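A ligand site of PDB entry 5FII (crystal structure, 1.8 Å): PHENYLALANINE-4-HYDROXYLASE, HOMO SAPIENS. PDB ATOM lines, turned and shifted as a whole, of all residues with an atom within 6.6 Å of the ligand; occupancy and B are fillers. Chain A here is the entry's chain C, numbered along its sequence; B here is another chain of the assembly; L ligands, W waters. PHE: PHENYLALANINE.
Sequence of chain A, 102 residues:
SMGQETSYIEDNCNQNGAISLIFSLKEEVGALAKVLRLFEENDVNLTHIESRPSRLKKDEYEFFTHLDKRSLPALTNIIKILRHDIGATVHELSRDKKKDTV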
ATOM      1  N   LEU A  25     -28.180 -15.899  15.751  1.00  0.00           N
ATOM      2  CA  LEU A  25     -29.548 -15.812  15.260  1.00  0.00           C
ATOM      3  C   LEU A  25     -30.225 -17.161  15.326  1.00  0.00           C
ATOM      4  O   LEU A  25     -29.569 -18.203  15.200  1.00  0.00           O
ATOM      5  CB  LEU A  25     -29.610 -15.348  13.805  1.00  0.00           C
ATOM      6  CG  LEU A  25     -28.960 -14.027  13.462  1.00  0.00           C
ATOM      7  CD1 LEU A  25     -29.137 -13.787  11.951  1.00  0.00           C
ATOM      8  CD2 LEU A  25     -29.581 -12.879  14.248  1.00  0.00           C
ATOM      9  N   LYS A  26     -31.547 -17.121  15.539  1.00  0.00           N
ATOM     10  CA  LYS A  26     -32.411 -18.283  15.386  1.00  0.00           C
ATOM     11  C   LYS A  26     -32.471 -18.712  13.931  1.00  0.00           C
ATOM     12  O   LYS A  26     -32.590 -17.865  13.052  1.00  0.00           O
ATOM     13  CB  LYS A  26     -33.811 -17.983  15.904  1.00  0.00           C
ATOM     14  CG  LYS A  26     -33.822 -17.879  17.426  1.00  0.00           C
ATOM     15  CD  LYS A  26     -35.206 -17.597  18.001  1.00  0.00           C
ATOM     16  CE  LYS A  26     -35.122 -17.431  19.511  1.00  0.00           C
ATOM     17  NZ  LYS A  26     -36.433 -17.643  20.203  1.00  0.00           N
ATOM     18  N   GLU A  27     -32.378 -20.006  13.698  1.00  0.00           N
ATOM     19  CA  GLU A  27     -32.388 -20.561  12.357  1.00  0.00           C
ATOM     20  C   GLU A  27     -33.758 -20.386  11.737  1.00  0.00           C
ATOM     21  O   GLU A  27     -34.781 -20.771  12.325  1.00  0.00           O
ATOM     22  CB  GLU A  27     -32.007 -22.040  12.370  1.00  0.00           C
ATOM     23  CG  GLU A  27     -32.349 -22.844  11.089  1.00  0.00           C
ATOM     24  CD  GLU A  27     -31.576 -22.411   9.852  1.00  0.00           C
ATOM     25  OE1 GLU A  27     -31.001 -21.302   9.800  1.00  0.00           O
ATOM     26  OE2 GLU A  27     -31.543 -23.205   8.893  1.00  0.00           O
ATOM     27  N   GLU A  28     -33.774 -19.742  10.578  1.00  0.00           N
ATOM     28  CA  GLU A  28     -34.972 -19.612   9.742  1.00  0.00           C
ATOM     29  C   GLU A  28     -34.548 -19.036   8.399  1.00  0.00           C
ATOM     30  O   GLU A  28     -33.517 -18.385   8.306  1.00  0.00           O
ATOM     31  CB  GLU A  28     -36.028 -18.698  10.378  1.00  0.00           C
ATOM     32  CG  GLU A  28     -35.585 -17.277  10.628  1.00  0.00           C
ATOM     33  CD  GLU A  28     -36.622 -16.461  11.368  1.00  0.00           C
ATOM     34  OE1 GLU A  28     -37.850 -16.647  11.158  1.00  0.00           O
ATOM     35  OE2 GLU A  28     -36.205 -15.612  12.171  1.00  0.00           O
ATOM     36  N   VAL A  29     -35.340 -19.274   7.363  1.00  0.00           N
ATOM     37  CA  VAL A  29     -35.061 -18.662   6.053  1.00  0.00           C
ATOM     38  C   VAL A  29     -35.067 -17.131   6.255  1.00  0.00           C
ATOM     39  O   VAL A  29     -35.957 -16.604   6.939  1.00  0.00           O
ATOM     40  CB  VAL A  29     -36.103 -19.059   5.007  1.00  0.00           C
ATOM     41  CG1 VAL A  29     -35.953 -18.249   3.718  1.00  0.00           C
ATOM     42  CG2 VAL A  29     -36.009 -20.562   4.715  1.00  0.00           C
ATOM     43  N   GLY A  30     -34.061 -16.460   5.697  1.00  0.00           N
ATOM     44  CA  GLY A  30     -34.004 -14.994   5.717  1.00  0.00           C
ATOM     45  C   GLY A  30     -33.542 -14.369   7.023  1.00  0.00           C
ATOM     46  O   GLY A  30     -33.583 -13.154   7.146  1.00  0.00           O
ATOM     47  N   ALA A  31     -33.033 -15.179   7.941  1.00  0.00           N
ATOM     48  CA  ALA A  31     -32.540 -14.709   9.245  1.00  0.00           C
ATOM     49  C   ALA A  31     -31.442 -13.677   9.054  1.00  0.00           C
ATOM     50  O   ALA A  31     -31.534 -12.568   9.566  1.00  0.00           O
ATOM     51  CB  ALA A  31     -32.022 -15.871  10.060  1.00  0.00           C
ATOM     52  N   LEU A  32     -30.436 -14.042   8.268  1.00  0.00           N
ATOM     53  CA  LEU A  32     -29.308 -13.142   8.035  1.00  0.00           C
ATOM     54  C   LEU A  32     -29.666 -11.923   7.169  1.00  0.00           C
ATOM     55  O   LEU A  32     -29.247 -10.795   7.470  1.00  0.00           O
ATOM     56  CB  LEU A  32     -28.110 -13.927   7.473  1.00  0.00           C
ATOM     57  CG  LEU A  32     -26.822 -13.111   7.339  1.00  0.00           C
ATOM     58  CD1 LEU A  32     -26.352 -12.548   8.671  1.00  0.00           C
ATOM     59  CD2 LEU A  32     -25.728 -13.978   6.719  1.00  0.00           C
ATOM     60  N   ALA A  33     -30.490 -12.131   6.159  1.00  0.00           N
ATOM     61  CA  ALA A  33     -30.998 -11.056   5.314  1.00  0.00           C
ATOM     62  C   ALA A  33     -31.596  -9.898   6.125  1.00  0.00           C
ATOM     63  O   ALA A  33     -31.367  -8.732   5.811  1.00  0.00           O
ATOM     64  CB  ALA A  33     -32.062 -11.598   4.370  1.00  0.00           C
ATOM     65  N   SER A  51     -20.051 -17.744   9.361  1.00  0.00           N
ATOM     66  CA  SER A  51     -21.030 -18.408  10.213  1.00  0.00           C
ATOM     67  C   SER A  51     -20.499 -19.723  10.754  1.00  0.00           C
ATOM     68  O   SER A  51     -19.580 -20.307  10.193  1.00  0.00           O
ATOM     69  CB  SER A  51     -22.307 -18.711   9.444  1.00  0.00           C
ATOM     70  OG  SER A  51     -22.079 -19.672   8.435  1.00  0.00           O
ATOM     71  N   ARG A  52     -21.170 -20.184  11.796  1.00  0.00           N
ATOM     72  CA  ARG A  52     -20.941 -21.479  12.394  1.00  0.00           C
ATOM     73  C   ARG A  52     -22.239 -21.939  13.058  1.00  0.00           C
ATOM     74  O   ARG A  52     -22.876 -21.141  13.744  1.00  0.00           O
ATOM     75  CB  ARG A  52     -19.887 -21.316  13.475  1.00  0.00           C
ATOM     76  CG  ARG A  52     -19.253 -22.587  13.935  1.00  0.00           C
ATOM     77  CD  ARG A  52     -18.077 -22.258  14.827  1.00  0.00           C
ATOM     78  NE  ARG A  52     -18.464 -21.555  16.067  1.00  0.00           N
ATOM     79  CZ  ARG A  52     -17.612 -20.890  16.845  1.00  0.00           C
ATOM     80  NH1 ARG A  52     -16.326 -20.789  16.526  1.00  0.00           N
ATOM     81  NH2 ARG A  52     -18.051 -20.290  17.944  1.00  0.00           N
ATOM     82  N   TYR A  61     -27.421 -20.147  14.786  1.00  0.00           N
ATOM     83  CA  TYR A  61     -26.130 -19.956  14.158  1.00  0.00           C
ATOM     84  C   TYR A  61     -25.426 -18.769  14.786  1.00  0.00           C
ATOM     85  O   TYR A  61     -26.084 -17.798  15.154  1.00  0.00           O
ATOM     86  CB  TYR A  61     -26.295 -19.699  12.669  1.00  0.00           C
ATOM     87  CG  TYR A  61     -26.510 -20.923  11.861  1.00  0.00           C
ATOM     88  CD1 TYR A  61     -27.797 -21.386  11.620  1.00  0.00           C
ATOM     89  CD2 TYR A  61     -25.436 -21.605  11.291  1.00  0.00           C
ATOM     90  CE1 TYR A  61     -27.993 -22.528  10.848  1.00  0.00           C
ATOM     91  CE2 TYR A  61     -25.635 -22.756  10.541  1.00  0.00           C
ATOM     92  CZ  TYR A  61     -26.932 -23.201  10.310  1.00  0.00           C
ATOM     93  OH  TYR A  61     -27.152 -24.330   9.532  1.00  0.00           O
ATOM     94  N   PHE A  63     -22.564 -15.788  14.176  1.00  0.00           N
ATOM     95  CA  PHE A  63     -21.981 -14.992  13.123  1.00  0.00           C
ATOM     96  C   PHE A  63     -20.860 -14.130  13.663  1.00  0.00           C
ATOM     97  O   PHE A  63     -21.039 -13.413  14.671  1.00  0.00           O
ATOM     98  CB  PHE A  63     -23.060 -14.145  12.443  1.00  0.00           C
ATOM     99  CG  PHE A  63     -24.146 -14.949  11.828  1.00  0.00           C
ATOM    100  CD1 PHE A  63     -25.256 -15.327  12.574  1.00  0.00           C
ATOM    101  CD2 PHE A  63     -24.047 -15.404  10.501  1.00  0.00           C
ATOM    102  CE1 PHE A  63     -26.256 -16.098  12.014  1.00  0.00           C
ATOM    103  CE2 PHE A  63     -25.054 -16.170   9.947  1.00  0.00           C
ATOM    104  CZ  PHE A  63     -26.152 -16.520  10.706  1.00  0.00           C
ATOM    105  N   LEU B  36     -28.811 -11.843  -0.340  1.00  0.00           N
ATOM    106  CA  LEU B  36     -29.573 -12.611   0.633  1.00  0.00           C
ATOM    107  C   LEU B  36     -31.052 -12.370   0.506  1.00  0.00           C
ATOM    108  O   LEU B  36     -31.826 -13.261   0.731  1.00  0.00           O
ATOM    109  CB  LEU B  36     -29.103 -12.376   2.074  1.00  0.00           C
ATOM    110  CG  LEU B  36     -27.638 -12.728   2.403  1.00  0.00           C
ATOM    111  CD1 LEU B  36     -27.364 -12.736   3.899  1.00  0.00           C
ATOM    112  CD2 LEU B  36     -27.234 -14.070   1.792  1.00  0.00           C
ATOM    113  N   VAL B  44     -34.421 -19.976  -0.564  1.00  0.00           N
ATOM    114  CA  VAL B  44     -33.089 -20.547  -0.433  1.00  0.00           C
ATOM    115  C   VAL B  44     -32.638 -20.301   1.010  1.00  0.00           C
ATOM    116  O   VAL B  44     -32.810 -19.205   1.517  1.00  0.00           O
ATOM    117  CB  VAL B  44     -32.101 -19.894  -1.435  1.00  0.00           C
ATOM    118  CG1 VAL B  44     -30.641 -20.174  -1.096  1.00  0.00           C
ATOM    119  CG2 VAL B  44     -32.423 -20.348  -2.855  1.00  0.00           C
ATOM    120  N   ASN B  45     -32.028 -21.314   1.626  1.00  0.00           N
ATOM    121  CA  ASN B  45     -31.676 -21.265   3.035  1.00  0.00           C
ATOM    122  C   ASN B  45     -30.226 -21.660   3.207  1.00  0.00           C
ATOM    123  O   ASN B  45     -29.795 -22.704   2.734  1.00  0.00           O
ATOM    124  CB  ASN B  45     -32.599 -22.179   3.845  1.00  0.00           C
ATOM    125  CG  ASN B  45     -32.381 -22.030   5.346  1.00  0.00           C
ATOM    126  OD1 ASN B  45     -32.467 -20.924   5.889  1.00  0.00           O
ATOM    127  ND2 ASN B  45     -32.058 -23.135   6.015  1.00  0.00           N
ATOM    128  N   LEU B  46     -29.456 -20.806   3.871  1.00  0.00           N
ATOM    129  CA  LEU B  46     -28.014 -21.005   3.972  1.00  0.00           C
ATOM    130  C   LEU B  46     -27.682 -21.845   5.158  1.00  0.00           C
ATOM    131  O   LEU B  46     -28.357 -21.722   6.198  1.00  0.00           O
ATOM    132  CB  LEU B  46     -27.295 -19.649   4.108  1.00  0.00           C
ATOM    133  CG  LEU B  46     -27.119 -18.912   2.783  1.00  0.00           C
ATOM    134  CD1 LEU B  46     -28.451 -18.423   2.229  1.00  0.00           C
ATOM    135  CD2 LEU B  46     -26.187 -17.728   2.976  1.00  0.00           C
ATOM    136  N   THR B  47     -26.679 -22.713   5.014  1.00  0.00           N
ATOM    137  CA  THR B  47     -26.114 -23.431   6.161  1.00  0.00           C
ATOM    138  C   THR B  47     -24.707 -22.985   6.507  1.00  0.00           C
ATOM    139  O   THR B  47     -24.212 -23.348   7.556  1.00  0.00           O
ATOM    140  CB  THR B  47     -26.125 -24.952   5.947  1.00  0.00           C
ATOM    141  OG1 THR B  47     -25.342 -25.265   4.793  1.00  0.00           O
ATOM    142  CG2 THR B  47     -27.539 -25.436   5.736  1.00  0.00           C
ATOM    143  N   HIS B  48     -24.064 -22.228   5.623  1.00  0.00           N
ATOM    144  CA  HIS B  48     -22.734 -21.708   5.879  1.00  0.00           C
ATOM    145  C   HIS B  48     -22.466 -20.504   4.987  1.00  0.00           C
ATOM    146  O   HIS B  48     -22.918 -20.477   3.832  1.00  0.00           O
ATOM    147  CB  HIS B  48     -21.698 -22.814   5.650  1.00  0.00           C
ATOM    148  CG  HIS B  48     -20.286 -22.357   5.749  1.00  0.00           C
ATOM    149  ND1 HIS B  48     -19.624 -22.247   6.953  1.00  0.00           N
ATOM    150  CD2 HIS B  48     -19.421 -21.953   4.795  1.00  0.00           C
ATOM    151  CE1 HIS B  48     -18.398 -21.800   6.728  1.00  0.00           C
ATOM    152  NE2 HIS B  48     -18.254 -21.616   5.423  1.00  0.00           N
ATOM    153  N   ILE B  49     -21.785 -19.501   5.542  1.00  0.00           N
ATOM    154  CA  ILE B  49     -21.212 -18.416   4.752  1.00  0.00           C
ATOM    155  C   ILE B  49     -19.847 -17.998   5.268  1.00  0.00           C
ATOM    156  O   ILE B  49     -19.587 -18.020   6.473  1.00  0.00           O
ATOM    157  CB  ILE B  49     -22.149 -17.182   4.618  1.00  0.00           C
ATOM    158  CG1 ILE B  49     -21.603 -16.170   3.622  1.00  0.00           C
ATOM    159  CG2 ILE B  49     -22.450 -16.523   5.974  1.00  0.00           C
ATOM    160  CD1 ILE B  49     -22.665 -15.212   3.104  1.00  0.00           C
ATOM    161  N   HIS B  66     -22.742 -22.566   1.749  1.00  0.00           N
ATOM    162  CA  HIS B  66     -23.495 -23.812   1.628  1.00  0.00           C
ATOM    163  C   HIS B  66     -24.995 -23.505   1.720  1.00  0.00           C
ATOM    164  O   HIS B  66     -25.430 -22.666   2.540  1.00  0.00           O
ATOM    165  CB  HIS B  66     -23.130 -24.811   2.704  1.00  0.00           C
ATOM    166  CG  HIS B  66     -21.764 -25.400   2.539  1.00  0.00           C
ATOM    167  ND1 HIS B  66     -20.910 -25.630   3.600  1.00  0.00           N
ATOM    168  CD2 HIS B  66     -21.116 -25.830   1.441  1.00  0.00           C
ATOM    169  CE1 HIS B  66     -19.791 -26.172   3.150  1.00  0.00           C
ATOM    170  NE2 HIS B  66     -19.885 -26.292   1.836  1.00  0.00           N
ATOM    171  N   ASP B  68     -28.909 -25.503   2.050  1.00  0.00           N
ATOM    172  CA  ASP B  68     -29.547 -26.762   2.380  1.00  0.00           C
ATOM    173  C   ASP B  68     -30.206 -27.424   1.151  1.00  0.00           C
ATOM    174  O   ASP B  68     -30.456 -26.773   0.115  1.00  0.00           O
ATOM    175  CB  ASP B  68     -30.491 -26.633   3.609  1.00  0.00           C
ATOM    176  CG  ASP B  68     -31.752 -25.819   3.364  1.00  0.00           C
ATOM    177  OD1 ASP B  68     -32.091 -25.465   2.236  1.00  0.00           O
ATOM    178  OD2 ASP B  68     -32.473 -25.579   4.380  1.00  0.00           O
HETATM  179  N   PHE L   1     -30.238 -20.271   7.506  1.00  0.00           N
HETATM  180  CA  PHE L   1     -30.288 -18.828   7.792  1.00  0.00           C
HETATM  181  C   PHE L   1     -30.358 -17.951   6.563  1.00  0.00           C
HETATM  182  O   PHE L   1     -30.263 -18.421   5.411  1.00  0.00           O
HETATM  183  CB  PHE L   1     -29.104 -18.411   8.681  1.00  0.00           C
HETATM  184  CG  PHE L   1     -27.734 -18.629   8.073  1.00  0.00           C
HETATM  185  CD1 PHE L   1     -27.182 -17.682   7.233  1.00  0.00           C
HETATM  186  CD2 PHE L   1     -26.960 -19.741   8.450  1.00  0.00           C
HETATM  187  CE1 PHE L   1     -25.899 -17.873   6.693  1.00  0.00           C
HETATM  188  CE2 PHE L   1     -25.695 -19.943   7.930  1.00  0.00           C
HETATM  189  CZ  PHE L   1     -25.160 -19.001   7.051  1.00  0.00           C
HETATM  190  OXT PHE L   1     -30.473 -16.706   6.689  1.00  0.00           O
HETATM  191  O   HOH W   1     -31.975 -17.510   3.712  1.00  0.00           O
HETATM  192  O   HOH W   2     -30.713 -14.675   5.037  1.00  0.00           O
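N of the ligand lies within salt-bridge range of OE1 of Glu 27. The backbone NH of Leu 46 of chain B lies within hydrogen-bond range of an oxygen (O) of the ligand, 3.0 Å away. The backbone carbonyl oxygen of Leu 46 of chain B lies within hydrogen-bond range of a nitrogen (N) of the ligand (2.7 Å). N of the ligand sits at hydrogen-bond distance from OD1 of Asn 45 of chain B, at 2.8 Å. An oxygen (OXT) of the ligand lies within hydrogen-bond range of the backbone NH of Leu 32, at 3.1 Å. The backbone NH of Ala 31 lies within hydrogen-bond range of an oxygen (OXT) of the ligand (3.2 Å).
Water W1 lies within hydrogen-bond range of O of the ligand (2.6 Å), O of Val 44 of chain B (2.9 Å) and N of Gly 30 (3.1 Å). Water W2 lies within hydrogen-bond range of an oxygen (OXT) of the ligand, the backbone NH (N) of Ala 33 and the backbone NH (N) of Leu 32.
Glu 28 touches the ligand (O to CA, 3.3 Å). N of Gly 30 touches OXT of the ligand, 3.7 Å away. OG of Ser 51 touches CZ of the ligand, at 3.4 Å. CG of Tyr 61 touches CD2 of the ligand (3.6 Å). CZ of Phe 63 touches CG of the ligand (3.7 Å). Thr 47 of chain B touches the ligand (C to CE2, 3.5 Å). His 48 of chain B touches the ligand. N of Ile 49 of chain B touches CZ of the ligand, at 3.7 Å. Along chain A the residues within 4 Å of the ligand span positions 27 to 63.
OE2 of Glu 27 is in hydrogen-bond range of ND2 of Asn 45 of chain B (2.9 Å). The side-chain amide nitrogen (ND2) of Asn 45 of chain B lies within hydrogen-bond range of the side-chain carboxylate (OD2) of Asp 68 of chain B, at 3.0 Å. The side-chain hydroxyl (OG) of Ser 51 lies within hydrogen-bond range of the backbone NH (N) of Ile 49 of chain B (2.9 Å). N of Thr 47 of chain B sits at hydrogen-bond distance from O of His 66 of chain B, at 2.8 Å. O of His 48 of chain B lies within hydrogen-bond range of N of His 66 of chain B (3.0 Å). The backbone carbonyl oxygen (O) of Tyr 61 is in hydrogen-bond range of the backbone NH (N) of Leu 25 (2.9 Å).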
